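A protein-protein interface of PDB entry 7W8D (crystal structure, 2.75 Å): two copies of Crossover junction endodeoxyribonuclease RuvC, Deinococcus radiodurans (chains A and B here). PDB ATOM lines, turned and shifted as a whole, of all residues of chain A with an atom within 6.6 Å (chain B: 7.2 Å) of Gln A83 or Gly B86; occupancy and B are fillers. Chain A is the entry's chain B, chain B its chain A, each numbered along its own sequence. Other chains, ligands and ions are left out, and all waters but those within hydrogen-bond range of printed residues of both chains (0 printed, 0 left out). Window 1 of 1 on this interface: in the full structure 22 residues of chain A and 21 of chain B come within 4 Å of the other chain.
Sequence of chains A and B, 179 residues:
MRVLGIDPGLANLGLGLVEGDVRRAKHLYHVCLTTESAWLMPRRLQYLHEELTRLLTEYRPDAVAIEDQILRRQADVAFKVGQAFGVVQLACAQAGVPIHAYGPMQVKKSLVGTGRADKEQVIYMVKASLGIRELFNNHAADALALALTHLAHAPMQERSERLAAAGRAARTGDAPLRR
The backbone NH (N) of Gln B83 sits close to the backbone carbonyl oxygen (O) of Gly A82 (3.4 Å).
NE2 of Gln B89 lies within hydrogen-bond range of OE1 of Gln A83 (2.5 Å).
Among the printed residues, pairs that only touch across the chains: Met A41 with Gln B89 (3.3 Å), Pro A42 with Gln B89 (3.8 Å), Leu A45 with Gly B86 (3.0 Å), Leu A45 with Leu B90 (3.6 Å), Ala A78 with Phe B79 (3.3 Å), Phe A79 with Arg B72 (3.9 Å), Phe A79 with Ala B78 (3.5 Å), Phe A79 with Val B81 (3.5 Å), Phe A79 with Gly B82 (3.7 Å), Phe A79 with Phe B85 (3.4 Å), Gly A82 with Phe B79 (3.4 Å), Gly A82 with Gly B82 (3.6 Å), Gln A83 with Gly B82 (3.3 Å), Gln A83 with Phe B85 (3.8 Å), Gln A83 with Gly B86 (3.9 Å), Phe A85 with Phe B79 (3.3 Å), Phe A85 with Gln B83 (3.5 Å), Gly A86 with Leu B45 (3.8 Å), Gly A86 with Gln B83 (3.9 Å), Gly A86 with Val B87 (3.7 Å) and Val A87 with Gly B86 (3.7 Å).
Of chain B, only Gly B82, Phe B85, Gly B86 and Gln B89 come within 4 Å of Gln A83.
Of chain A, only Leu A45 (3.0 Å), Gln A83 (3.9 Å) and Val A87 (3.7 Å) come within 4 Å of Gly B86.
Of the printed residues of chain A, Val B87 touches Gly A86.
Printed residues of chain A within 4 Å of Leu B90: Leu A45.
Ala B84 touches none of the printed residues of chain A.
Val A88 touches none of the printed residues of chain B.
The nearest residue of chain A that does not touch Gly B86 is Ala A84 (5.8 Å).
The nearest printed residue of chain B that does not touch Val A87 is Leu B90 (4.03 Å).
Printed residues of chain A that touch a printed residue of chain B: Met A41, Pro A42, Leu A45, Ala A78, Phe A79, Gly A82, Gln A83, Phe A85, Gly A86 and Val A87.
Hydrophobic or aromatic side chains of chain A that line the printed part of chain B: Met A41, Pro A42, Leu A45, Phe A79, Phe A85 and Val A87.
Of the 17 printed residues of chain B, 12 touch a printed residue of chain A.
Along chain B the printed residues that touch a printed residue of chain A span positions 45 to 90.
Ala A78 touches Phe B79, and with the chains exchanged Phe A79 touches Ala B78.
Phe A79 touches Gly B82, and with the chains exchanged Gly A82 touches Phe B79.
Phe A79 touches Phe B85, and with the chains exchanged Phe A85 touches Phe B79.
Gly B82 touches its own counterpart, Gly A82.
Positions printed for both chains: 45, 78, 79, 81, 82, 83, 84, 85, 86, 87 and 88.
Of the 23 pairs that touch across the chains among the printed residues, 17 have their exchanged pair printed and touching as well.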
ATOM      1  N   LEU A  10     -31.667 -27.001  18.426  1.00  0.00           N
ATOM      2  CA  LEU A  10     -32.034 -25.838  19.219  1.00  0.00           C
ATOM      3  C   LEU A  10     -33.153 -26.164  20.199  1.00  0.00           C
ATOM      4  O   LEU A  10     -33.010 -25.932  21.402  1.00  0.00           O
ATOM      5  CB  LEU A  10     -32.431 -24.683  18.298  1.00  0.00           C
ATOM      6  CG  LEU A  10     -32.594 -23.353  19.019  1.00  0.00           C
ATOM      7  CD1 LEU A  10     -31.863 -22.277  18.256  1.00  0.00           C
ATOM      8  CD2 LEU A  10     -34.056 -23.013  19.145  1.00  0.00           C
ATOM      9  N   MET A  41     -34.168 -15.834  21.020  1.00  0.00           N
ATOM     10  CA  MET A  41     -33.034 -16.624  20.548  1.00  0.00           C
ATOM     11  C   MET A  41     -31.816 -16.511  21.459  1.00  0.00           C
ATOM     12  O   MET A  41     -31.271 -17.557  21.843  1.00  0.00           O
ATOM     13  CB  MET A  41     -32.707 -16.234  19.101  1.00  0.00           C
ATOM     14  CG  MET A  41     -31.895 -17.283  18.381  1.00  0.00           C
ATOM     15  SD  MET A  41     -32.694 -18.895  18.449  1.00  0.00           S
ATOM     16  CE  MET A  41     -32.885 -19.227  16.704  1.00  0.00           C
ATOM     17  N   PRO A  42     -31.368 -15.318  21.878  1.00  0.00           N
ATOM     18  CA  PRO A  42     -30.191 -15.271  22.765  1.00  0.00           C
ATOM     19  C   PRO A  42     -30.381 -15.994  24.093  1.00  0.00           C
ATOM     20  O   PRO A  42     -29.433 -16.623  24.582  1.00  0.00           O
ATOM     21  CB  PRO A  42     -29.972 -13.764  22.961  1.00  0.00           C
ATOM     22  CG  PRO A  42     -30.582 -13.139  21.768  1.00  0.00           C
ATOM     23  CD  PRO A  42     -31.792 -13.962  21.484  1.00  0.00           C
ATOM     24  N   LEU A  45     -29.983 -19.586  23.390  1.00  0.00           N
ATOM     25  CA  LEU A  45     -28.561 -19.805  23.153  1.00  0.00           C
ATOM     26  C   LEU A  45     -27.767 -19.754  24.453  1.00  0.00           C
ATOM     27  O   LEU A  45     -26.784 -20.485  24.614  1.00  0.00           O
ATOM     28  CB  LEU A  45     -28.030 -18.771  22.163  1.00  0.00           C
ATOM     29  CG  LEU A  45     -28.043 -19.167  20.686  1.00  0.00           C
ATOM     30  CD1 LEU A  45     -29.448 -19.307  20.144  1.00  0.00           C
ATOM     31  CD2 LEU A  45     -27.282 -18.148  19.891  1.00  0.00           C
ATOM     32  N   ASP A  76     -35.129 -21.039   6.814  1.00  0.00           N
ATOM     33  CA  ASP A  76     -35.274 -20.411   8.125  1.00  0.00           C
ATOM     34  C   ASP A  76     -34.917 -21.387   9.238  1.00  0.00           C
ATOM     35  O   ASP A  76     -34.263 -21.013  10.218  1.00  0.00           O
ATOM     36  CB  ASP A  76     -36.694 -19.863   8.309  1.00  0.00           C
ATOM     37  CG  ASP A  76     -37.760 -20.951   8.294  1.00  0.00           C
ATOM     38  OD1 ASP A  76     -37.435 -22.116   7.979  1.00  0.00           O
ATOM     39  OD2 ASP A  76     -38.930 -20.638   8.602  1.00  0.00           O
ATOM     40  N   ALA A  78     -32.836 -23.932   8.878  1.00  0.00           N
ATOM     41  CA  ALA A  78     -31.393 -24.134   8.791  1.00  0.00           C
ATOM     42  C   ALA A  78     -30.634 -23.004   9.473  1.00  0.00           C
ATOM     43  O   ALA A  78     -29.577 -23.231  10.074  1.00  0.00           O
ATOM     44  CB  ALA A  78     -30.970 -24.262   7.327  1.00  0.00           C
ATOM     45  N   PHE A  79     -31.160 -21.780   9.394  1.00  0.00           N
ATOM     46  CA  PHE A  79     -30.537 -20.653  10.080  1.00  0.00           C
ATOM     47  C   PHE A  79     -30.674 -20.784  11.592  1.00  0.00           C
ATOM     48  O   PHE A  79     -29.713 -20.539  12.332  1.00  0.00           O
ATOM     49  CB  PHE A  79     -31.157 -19.346   9.581  1.00  0.00           C
ATOM     50  CG  PHE A  79     -30.541 -18.108  10.171  1.00  0.00           C
ATOM     51  CD1 PHE A  79     -29.408 -17.546   9.609  1.00  0.00           C
ATOM     52  CD2 PHE A  79     -31.110 -17.493  11.273  1.00  0.00           C
ATOM     53  CE1 PHE A  79     -28.847 -16.401  10.144  1.00  0.00           C
ATOM     54  CE2 PHE A  79     -30.551 -16.350  11.812  1.00  0.00           C
ATOM     55  CZ  PHE A  79     -29.419 -15.805  11.246  1.00  0.00           C
ATOM     56  N   LYS A  80     -31.862 -21.170  12.071  1.00  0.00           N
ATOM     57  CA  LYS A  80     -32.058 -21.379  13.503  1.00  0.00           C
ATOM     58  C   LYS A  80     -31.223 -22.545  14.018  1.00  0.00           C
ATOM     59  O   LYS A  80     -30.633 -22.461  15.101  1.00  0.00           O
ATOM     60  CB  LYS A  80     -33.538 -21.618  13.804  1.00  0.00           C
ATOM     61  CG  LYS A  80     -34.403 -20.375  13.748  1.00  0.00           C
ATOM     62  CD  LYS A  80     -35.828 -20.687  14.176  1.00  0.00           C
ATOM     63  CE  LYS A  80     -36.664 -19.422  14.265  1.00  0.00           C
ATOM     64  NZ  LYS A  80     -36.583 -18.621  13.010  1.00  0.00           N
ATOM     65  N   VAL A  81     -31.172 -23.645  13.265  1.00  0.00           N
ATOM     66  CA  VAL A  81     -30.349 -24.778  13.674  1.00  0.00           C
ATOM     67  C   VAL A  81     -28.870 -24.416  13.615  1.00  0.00           C
ATOM     68  O   VAL A  81     -28.081 -24.858  14.460  1.00  0.00           O
ATOM     69  CB  VAL A  81     -30.675 -26.012  12.808  1.00  0.00           C
ATOM     70  CG1 VAL A  81     -29.700 -27.146  13.092  1.00  0.00           C
ATOM     71  CG2 VAL A  81     -32.102 -26.472  13.059  1.00  0.00           C
ATOM     72  N   GLY A  82     -28.470 -23.597  12.640  1.00  0.00           N
ATOM     73  CA  GLY A  82     -27.079 -23.188  12.543  1.00  0.00           C
ATOM     74  C   GLY A  82     -26.610 -22.331  13.703  1.00  0.00           C
ATOM     75  O   GLY A  82     -25.433 -22.377  14.073  1.00  0.00           O
ATOM     76  N   GLN A  83     -27.512 -21.536  14.286  1.00  0.00           N
ATOM     77  CA  GLN A  83     -27.143 -20.722  15.441  1.00  0.00           C
ATOM     78  C   GLN A  83     -26.776 -21.587  16.637  1.00  0.00           C
ATOM     79  O   GLN A  83     -25.815 -21.287  17.354  1.00  0.00           O
ATOM     80  CB  GLN A  83     -28.284 -19.783  15.818  1.00  0.00           C
ATOM     81  CG  GLN A  83     -28.547 -18.686  14.826  1.00  0.00           C
ATOM     82  CD  GLN A  83     -29.732 -17.850  15.233  1.00  0.00           C
ATOM     83  OE1 GLN A  83     -29.697 -17.162  16.249  1.00  0.00           O
ATOM     84  NE2 GLN A  83     -30.802 -17.923  14.455  1.00  0.00           N
ATOM     85  N   ALA A  84     -27.553 -22.645  16.886  1.00  0.00           N
ATOM     86  CA  ALA A  84     -27.204 -23.581  17.948  1.00  0.00           C
ATOM     87  C   ALA A  84     -25.922 -24.332  17.625  1.00  0.00           C
ATOM     88  O   ALA A  84     -25.143 -24.640  18.533  1.00  0.00           O
ATOM     89  CB  ALA A  84     -28.350 -24.565  18.180  1.00  0.00           C
ATOM     90  N   PHE A  85     -25.684 -24.624  16.345  1.00  0.00           N
ATOM     91  CA  PHE A  85     -24.483 -25.356  15.959  1.00  0.00           C
ATOM     92  C   PHE A  85     -23.224 -24.541  16.231  1.00  0.00           C
ATOM     93  O   PHE A  85     -22.211 -25.088  16.685  1.00  0.00           O
ATOM     94  CB  PHE A  85     -24.569 -25.749  14.484  1.00  0.00           C
ATOM     95  CG  PHE A  85     -23.669 -26.891  14.108  1.00  0.00           C
ATOM     96  CD1 PHE A  85     -23.935 -28.172  14.560  1.00  0.00           C
ATOM     97  CD2 PHE A  85     -22.565 -26.685  13.297  1.00  0.00           C
ATOM     98  CE1 PHE A  85     -23.113 -29.226  14.215  1.00  0.00           C
ATOM     99  CE2 PHE A  85     -21.740 -27.735  12.946  1.00  0.00           C
ATOM    100  CZ  PHE A  85     -22.014 -29.008  13.407  1.00  0.00           C
ATOM    101  N   GLY A  86     -23.264 -23.235  15.963  1.00  0.00           N
ATOM    102  CA  GLY A  86     -22.104 -22.400  16.232  1.00  0.00           C
ATOM    103  C   GLY A  86     -21.830 -22.243  17.716  1.00  0.00           C
ATOM    104  O   GLY A  86     -20.674 -22.182  18.140  1.00  0.00           O
ATOM    105  N   VAL A  87     -22.890 -22.177  18.524  1.00  0.00           N
ATOM    106  CA  VAL A  87     -22.731 -22.061  19.969  1.00  0.00           C
ATOM    107  C   VAL A  87     -22.193 -23.362  20.559  1.00  0.00           C
ATOM    108  O   VAL A  87     -21.479 -23.349  21.571  1.00  0.00           O
ATOM    109  CB  VAL A  87     -24.074 -21.630  20.592  1.00  0.00           C
ATOM    110  CG1 VAL A  87     -24.173 -22.035  22.052  1.00  0.00           C
ATOM    111  CG2 VAL A  87     -24.255 -20.121  20.439  1.00  0.00           C
ATOM    112  N   VAL A  88     -22.493 -24.498  19.926  1.00  0.00           N
ATOM    113  CA  VAL A  88     -21.893 -25.761  20.344  1.00  0.00           C
ATOM    114  C   VAL A  88     -20.430 -25.823  19.919  1.00  0.00           C
ATOM    115  O   VAL A  88     -19.561 -26.235  20.697  1.00  0.00           O
ATOM    116  CB  VAL A  88     -22.703 -26.943  19.782  1.00  0.00           C
ATOM    117  CG1 VAL A  88     -21.939 -28.242  19.945  1.00  0.00           C
ATOM    118  CG2 VAL A  88     -24.045 -27.034  20.481  1.00  0.00           C
ATOM    119  N   LEU B  45     -15.120 -18.992  15.221  1.00  0.00           N
ATOM    120  CA  LEU B  45     -16.219 -18.579  16.084  1.00  0.00           C
ATOM    121  C   LEU B  45     -15.744 -18.227  17.486  1.00  0.00           C
ATOM    122  O   LEU B  45     -16.462 -17.535  18.216  1.00  0.00           O
ATOM    123  CB  LEU B  45     -17.274 -19.683  16.159  1.00  0.00           C
ATOM    124  CG  LEU B  45     -17.878 -20.168  14.841  1.00  0.00           C
ATOM    125  CD1 LEU B  45     -18.515 -21.535  15.044  1.00  0.00           C
ATOM    126  CD2 LEU B  45     -18.905 -19.189  14.313  1.00  0.00           C
ATOM    127  N   HIS B  49     -16.247 -14.335  18.907  1.00  0.00           N
ATOM    128  CA  HIS B  49     -16.842 -14.265  20.237  1.00  0.00           C
ATOM    129  C   HIS B  49     -15.912 -13.580  21.224  1.00  0.00           C
ATOM    130  O   HIS B  49     -16.377 -12.906  22.148  1.00  0.00           O
ATOM    131  CB  HIS B  49     -17.188 -15.659  20.757  1.00  0.00           C
ATOM    132  CG  HIS B  49     -17.856 -15.644  22.096  1.00  0.00           C
ATOM    133  ND1 HIS B  49     -17.150 -15.689  23.280  1.00  0.00           N
ATOM    134  CD2 HIS B  49     -19.163 -15.568  22.440  1.00  0.00           C
ATOM    135  CE1 HIS B  49     -17.996 -15.646  24.294  1.00  0.00           C
ATOM    136  NE2 HIS B  49     -19.224 -15.574  23.812  1.00  0.00           N
ATOM    137  N   ARG B  72     -32.669 -15.481   1.830  1.00  0.00           N
ATOM    138  CA  ARG B  72     -33.514 -16.650   2.075  1.00  0.00           C
ATOM    139  C   ARG B  72     -33.664 -17.565   0.856  1.00  0.00           C
ATOM    140  O   ARG B  72     -34.776 -17.902   0.447  1.00  0.00           O
ATOM    141  CB  ARG B  72     -34.892 -16.190   2.555  1.00  0.00           C
ATOM    142  CG  ARG B  72     -34.956 -15.880   4.043  1.00  0.00           C
ATOM    143  CD  ARG B  72     -34.480 -17.083   4.835  1.00  0.00           C
ATOM    144  NE  ARG B  72     -34.378 -16.795   6.258  1.00  0.00           N
ATOM    145  CZ  ARG B  72     -33.245 -16.481   6.874  1.00  0.00           C
ATOM    146  NH1 ARG B  72     -33.251 -16.236   8.176  1.00  0.00           N
ATOM    147  NH2 ARG B  72     -32.108 -16.423   6.195  1.00  0.00           N
ATOM    148  N   ALA B  78     -27.805 -20.631   4.664  1.00  0.00           N
ATOM    149  CA  ALA B  78     -28.335 -20.027   5.884  1.00  0.00           C
ATOM    150  C   ALA B  78     -27.764 -20.700   7.125  1.00  0.00           C
ATOM    151  O   ALA B  78     -27.515 -20.038   8.140  1.00  0.00           O
ATOM    152  CB  ALA B  78     -29.862 -20.097   5.889  1.00  0.00           C
ATOM    153  N   PHE B  79     -27.556 -22.016   7.063  1.00  0.00           N
ATOM    154  CA  PHE B  79     -26.920 -22.722   8.170  1.00  0.00           C
ATOM    155  C   PHE B  79     -25.515 -22.186   8.422  1.00  0.00           C
ATOM    156  O   PHE B  79     -25.143 -21.894   9.565  1.00  0.00           O
ATOM    157  CB  PHE B  79     -26.887 -24.223   7.879  1.00  0.00           C
ATOM    158  CG  PHE B  79     -26.139 -25.011   8.905  1.00  0.00           C
ATOM    159  CD1 PHE B  79     -24.783 -25.246   8.761  1.00  0.00           C
ATOM    160  CD2 PHE B  79     -26.786 -25.498  10.026  1.00  0.00           C
ATOM    161  CE1 PHE B  79     -24.089 -25.952   9.711  1.00  0.00           C
ATOM    162  CE2 PHE B  79     -26.097 -26.210  10.979  1.00  0.00           C
ATOM    163  CZ  PHE B  79     -24.745 -26.434  10.820  1.00  0.00           C
ATOM    164  N   VAL B  81     -24.348 -19.291   7.597  1.00  0.00           N
ATOM    165  CA  VAL B  81     -24.493 -17.933   8.115  1.00  0.00           C
ATOM    166  C   VAL B  81     -24.921 -17.958   9.578  1.00  0.00           C
ATOM    167  O   VAL B  81     -24.441 -17.160  10.393  1.00  0.00           O
ATOM    168  CB  VAL B  81     -25.490 -17.142   7.245  1.00  0.00           C
ATOM    169  CG1 VAL B  81     -26.061 -15.953   8.007  1.00  0.00           C
ATOM    170  CG2 VAL B  81     -24.824 -16.681   5.961  1.00  0.00           C
ATOM    171  N   GLY B  82     -25.816 -18.882   9.938  1.00  0.00           N
ATOM    172  CA  GLY B  82     -26.372 -18.891  11.281  1.00  0.00           C
ATOM    173  C   GLY B  82     -25.354 -19.152  12.373  1.00  0.00           C
ATOM    174  O   GLY B  82     -25.517 -18.676  13.501  1.00  0.00           O
ATOM    175  N   GLN B  83     -24.299 -19.913  12.065  1.00  0.00           N
ATOM    176  CA  GLN B  83     -23.280 -20.216  13.068  1.00  0.00           C
ATOM    177  C   GLN B  83     -22.615 -18.946  13.579  1.00  0.00           C
ATOM    178  O   GLN B  83     -22.449 -18.762  14.791  1.00  0.00           O
ATOM    179  CB  GLN B  83     -22.229 -21.160  12.486  1.00  0.00           C
ATOM    180  CG  GLN B  83     -22.760 -22.515  12.085  1.00  0.00           C
ATOM    181  CD  GLN B  83     -21.719 -23.343  11.364  1.00  0.00           C
ATOM    182  OE1 GLN B  83     -21.768 -23.499  10.144  1.00  0.00           O
ATOM    183  NE2 GLN B  83     -20.762 -23.871  12.112  1.00  0.00           N
ATOM    184  N   ALA B  84     -22.208 -18.063  12.662  1.00  0.00           N
ATOM    185  CA  ALA B  84     -21.653 -16.779  13.072  1.00  0.00           C
ATOM    186  C   ALA B  84     -22.690 -15.949  13.815  1.00  0.00           C
ATOM    187  O   ALA B  84     -22.388 -15.343  14.850  1.00  0.00           O
ATOM    188  CB  ALA B  84     -21.133 -16.018  11.853  1.00  0.00           C
ATOM    189  N   PHE B  85     -23.926 -15.929  13.309  1.00  0.00           N
ATOM    190  CA  PHE B  85     -24.976 -15.103  13.897  1.00  0.00           C
ATOM    191  C   PHE B  85     -25.259 -15.500  15.341  1.00  0.00           C
ATOM    192  O   PHE B  85     -25.494 -14.637  16.195  1.00  0.00           O
ATOM    193  CB  PHE B  85     -26.243 -15.209  13.050  1.00  0.00           C
ATOM    194  CG  PHE B  85     -27.239 -14.122  13.308  1.00  0.00           C
ATOM    195  CD1 PHE B  85     -28.341 -14.351  14.114  1.00  0.00           C
ATOM    196  CD2 PHE B  85     -27.081 -12.873  12.732  1.00  0.00           C
ATOM    197  CE1 PHE B  85     -29.265 -13.350  14.343  1.00  0.00           C
ATOM    198  CE2 PHE B  85     -27.998 -11.868  12.960  1.00  0.00           C
ATOM    199  CZ  PHE B  85     -29.090 -12.105  13.769  1.00  0.00           C
ATOM    200  N   GLY B  86     -25.231 -16.803  15.634  1.00  0.00           N
ATOM    201  CA  GLY B  86     -25.526 -17.263  16.981  1.00  0.00           C
ATOM    202  C   GLY B  86     -24.434 -16.970  17.986  1.00  0.00           C
ATOM    203  O   GLY B  86     -24.722 -16.698  19.155  1.00  0.00           O
ATOM    204  N   VAL B  87     -23.174 -17.030  17.560  1.00  0.00           N
ATOM    205  CA  VAL B  87     -22.083 -16.639  18.446  1.00  0.00           C
ATOM    206  C   VAL B  87     -22.171 -15.151  18.770  1.00  0.00           C
ATOM    207  O   VAL B  87     -21.879 -14.725  19.896  1.00  0.00           O
ATOM    208  CB  VAL B  87     -20.734 -17.023  17.809  1.00  0.00           C
ATOM    209  CG1 VAL B  87     -19.612 -16.199  18.385  1.00  0.00           C
ATOM    210  CG2 VAL B  87     -20.460 -18.505  18.018  1.00  0.00           C
ATOM    211  N   VAL B  88     -22.602 -14.342  17.802  1.00  0.00           N
ATOM    212  CA  VAL B  88     -22.785 -12.914  18.047  1.00  0.00           C
ATOM    213  C   VAL B  88     -23.939 -12.682  19.015  1.00  0.00           C
ATOM    214  O   VAL B  88     -23.839 -11.872  19.944  1.00  0.00           O
ATOM    215  CB  VAL B  88     -23.001 -12.166  16.720  1.00  0.00           C
ATOM    216  CG1 VAL B  88     -23.491 -10.753  16.980  1.00  0.00           C
ATOM    217  CG2 VAL B  88     -21.711 -12.143  15.916  1.00  0.00           C
ATOM    218  N   GLN B  89     -25.052 -13.393  18.817  1.00  0.00           N
ATOM    219  CA  GLN B  89     -26.206 -13.208  19.690  1.00  0.00           C
ATOM    220  C   GLN B  89     -25.905 -13.661  21.113  1.00  0.00           C
ATOM    221  O   GLN B  89     -26.391 -13.060  22.080  1.00  0.00           O
ATOM    222  CB  GLN B  89     -27.416 -13.957  19.131  1.00  0.00           C
ATOM    223  CG  GLN B  89     -27.949 -13.389  17.825  1.00  0.00           C
ATOM    224  CD  GLN B  89     -29.421 -13.691  17.610  1.00  0.00           C
ATOM    225  OE1 GLN B  89     -30.243 -12.779  17.522  1.00  0.00           O
ATOM    226  NE2 GLN B  89     -29.760 -14.972  17.514  1.00  0.00           N
ATOM    227  N   LEU B  90     -25.098 -14.716  21.263  1.00  0.00           N
ATOM    228  CA  LEU B  90     -24.786 -15.228  22.593  1.00  0.00           C
ATOM    229  C   LEU B  90     -23.919 -14.252  23.378  1.00  0.00           C
ATOM    230  O   LEU B  90     -24.139 -14.047  24.578  1.00  0.00           O
ATOM    231  CB  LEU B  90     -24.094 -16.587  22.482  1.00  0.00           C
ATOM    232  CG  LEU B  90     -23.463 -17.136  23.766  1.00  0.00           C
ATOM    233  CD1 LEU B  90     -24.506 -17.714  24.703  1.00  0.00           C
ATOM    234  CD2 LEU B  90     -22.405 -18.166  23.439  1.00  0.00           C
ATOM    235  N   ALA B  91     -22.922 -13.652  22.723  1.00  0.00           N
ATOM    236  CA  ALA B  91     -22.077 -12.672  23.400  1.00  0.00           C
ATOM    237  C   ALA B  91     -22.904 -11.516  23.945  1.00  0.00           C
ATOM    238  O   ALA B  91     -22.604 -10.978  25.017  1.00  0.00           O
ATOM    239  CB  ALA B  91     -21.003 -12.156  22.444  1.00  0.00           C
ATOM    240  N   CYS B  92     -23.959 -11.128  23.225  1.00  0.00           N
ATOM    241  CA  CYS B  92     -24.807 -10.036  23.686  1.00  0.00           C
ATOM    242  C   CYS B  92     -25.636 -10.458  24.892  1.00  0.00           C
ATOM    243  O   CYS B  92     -25.685  -9.748  25.902  1.00  0.00           O
ATOM    244  CB  CYS B  92     -25.704  -9.554  22.547  1.00  0.00           C
ATOM    245  SG  CYS B  92     -24.793  -8.921  21.114  1.00  0.00           S
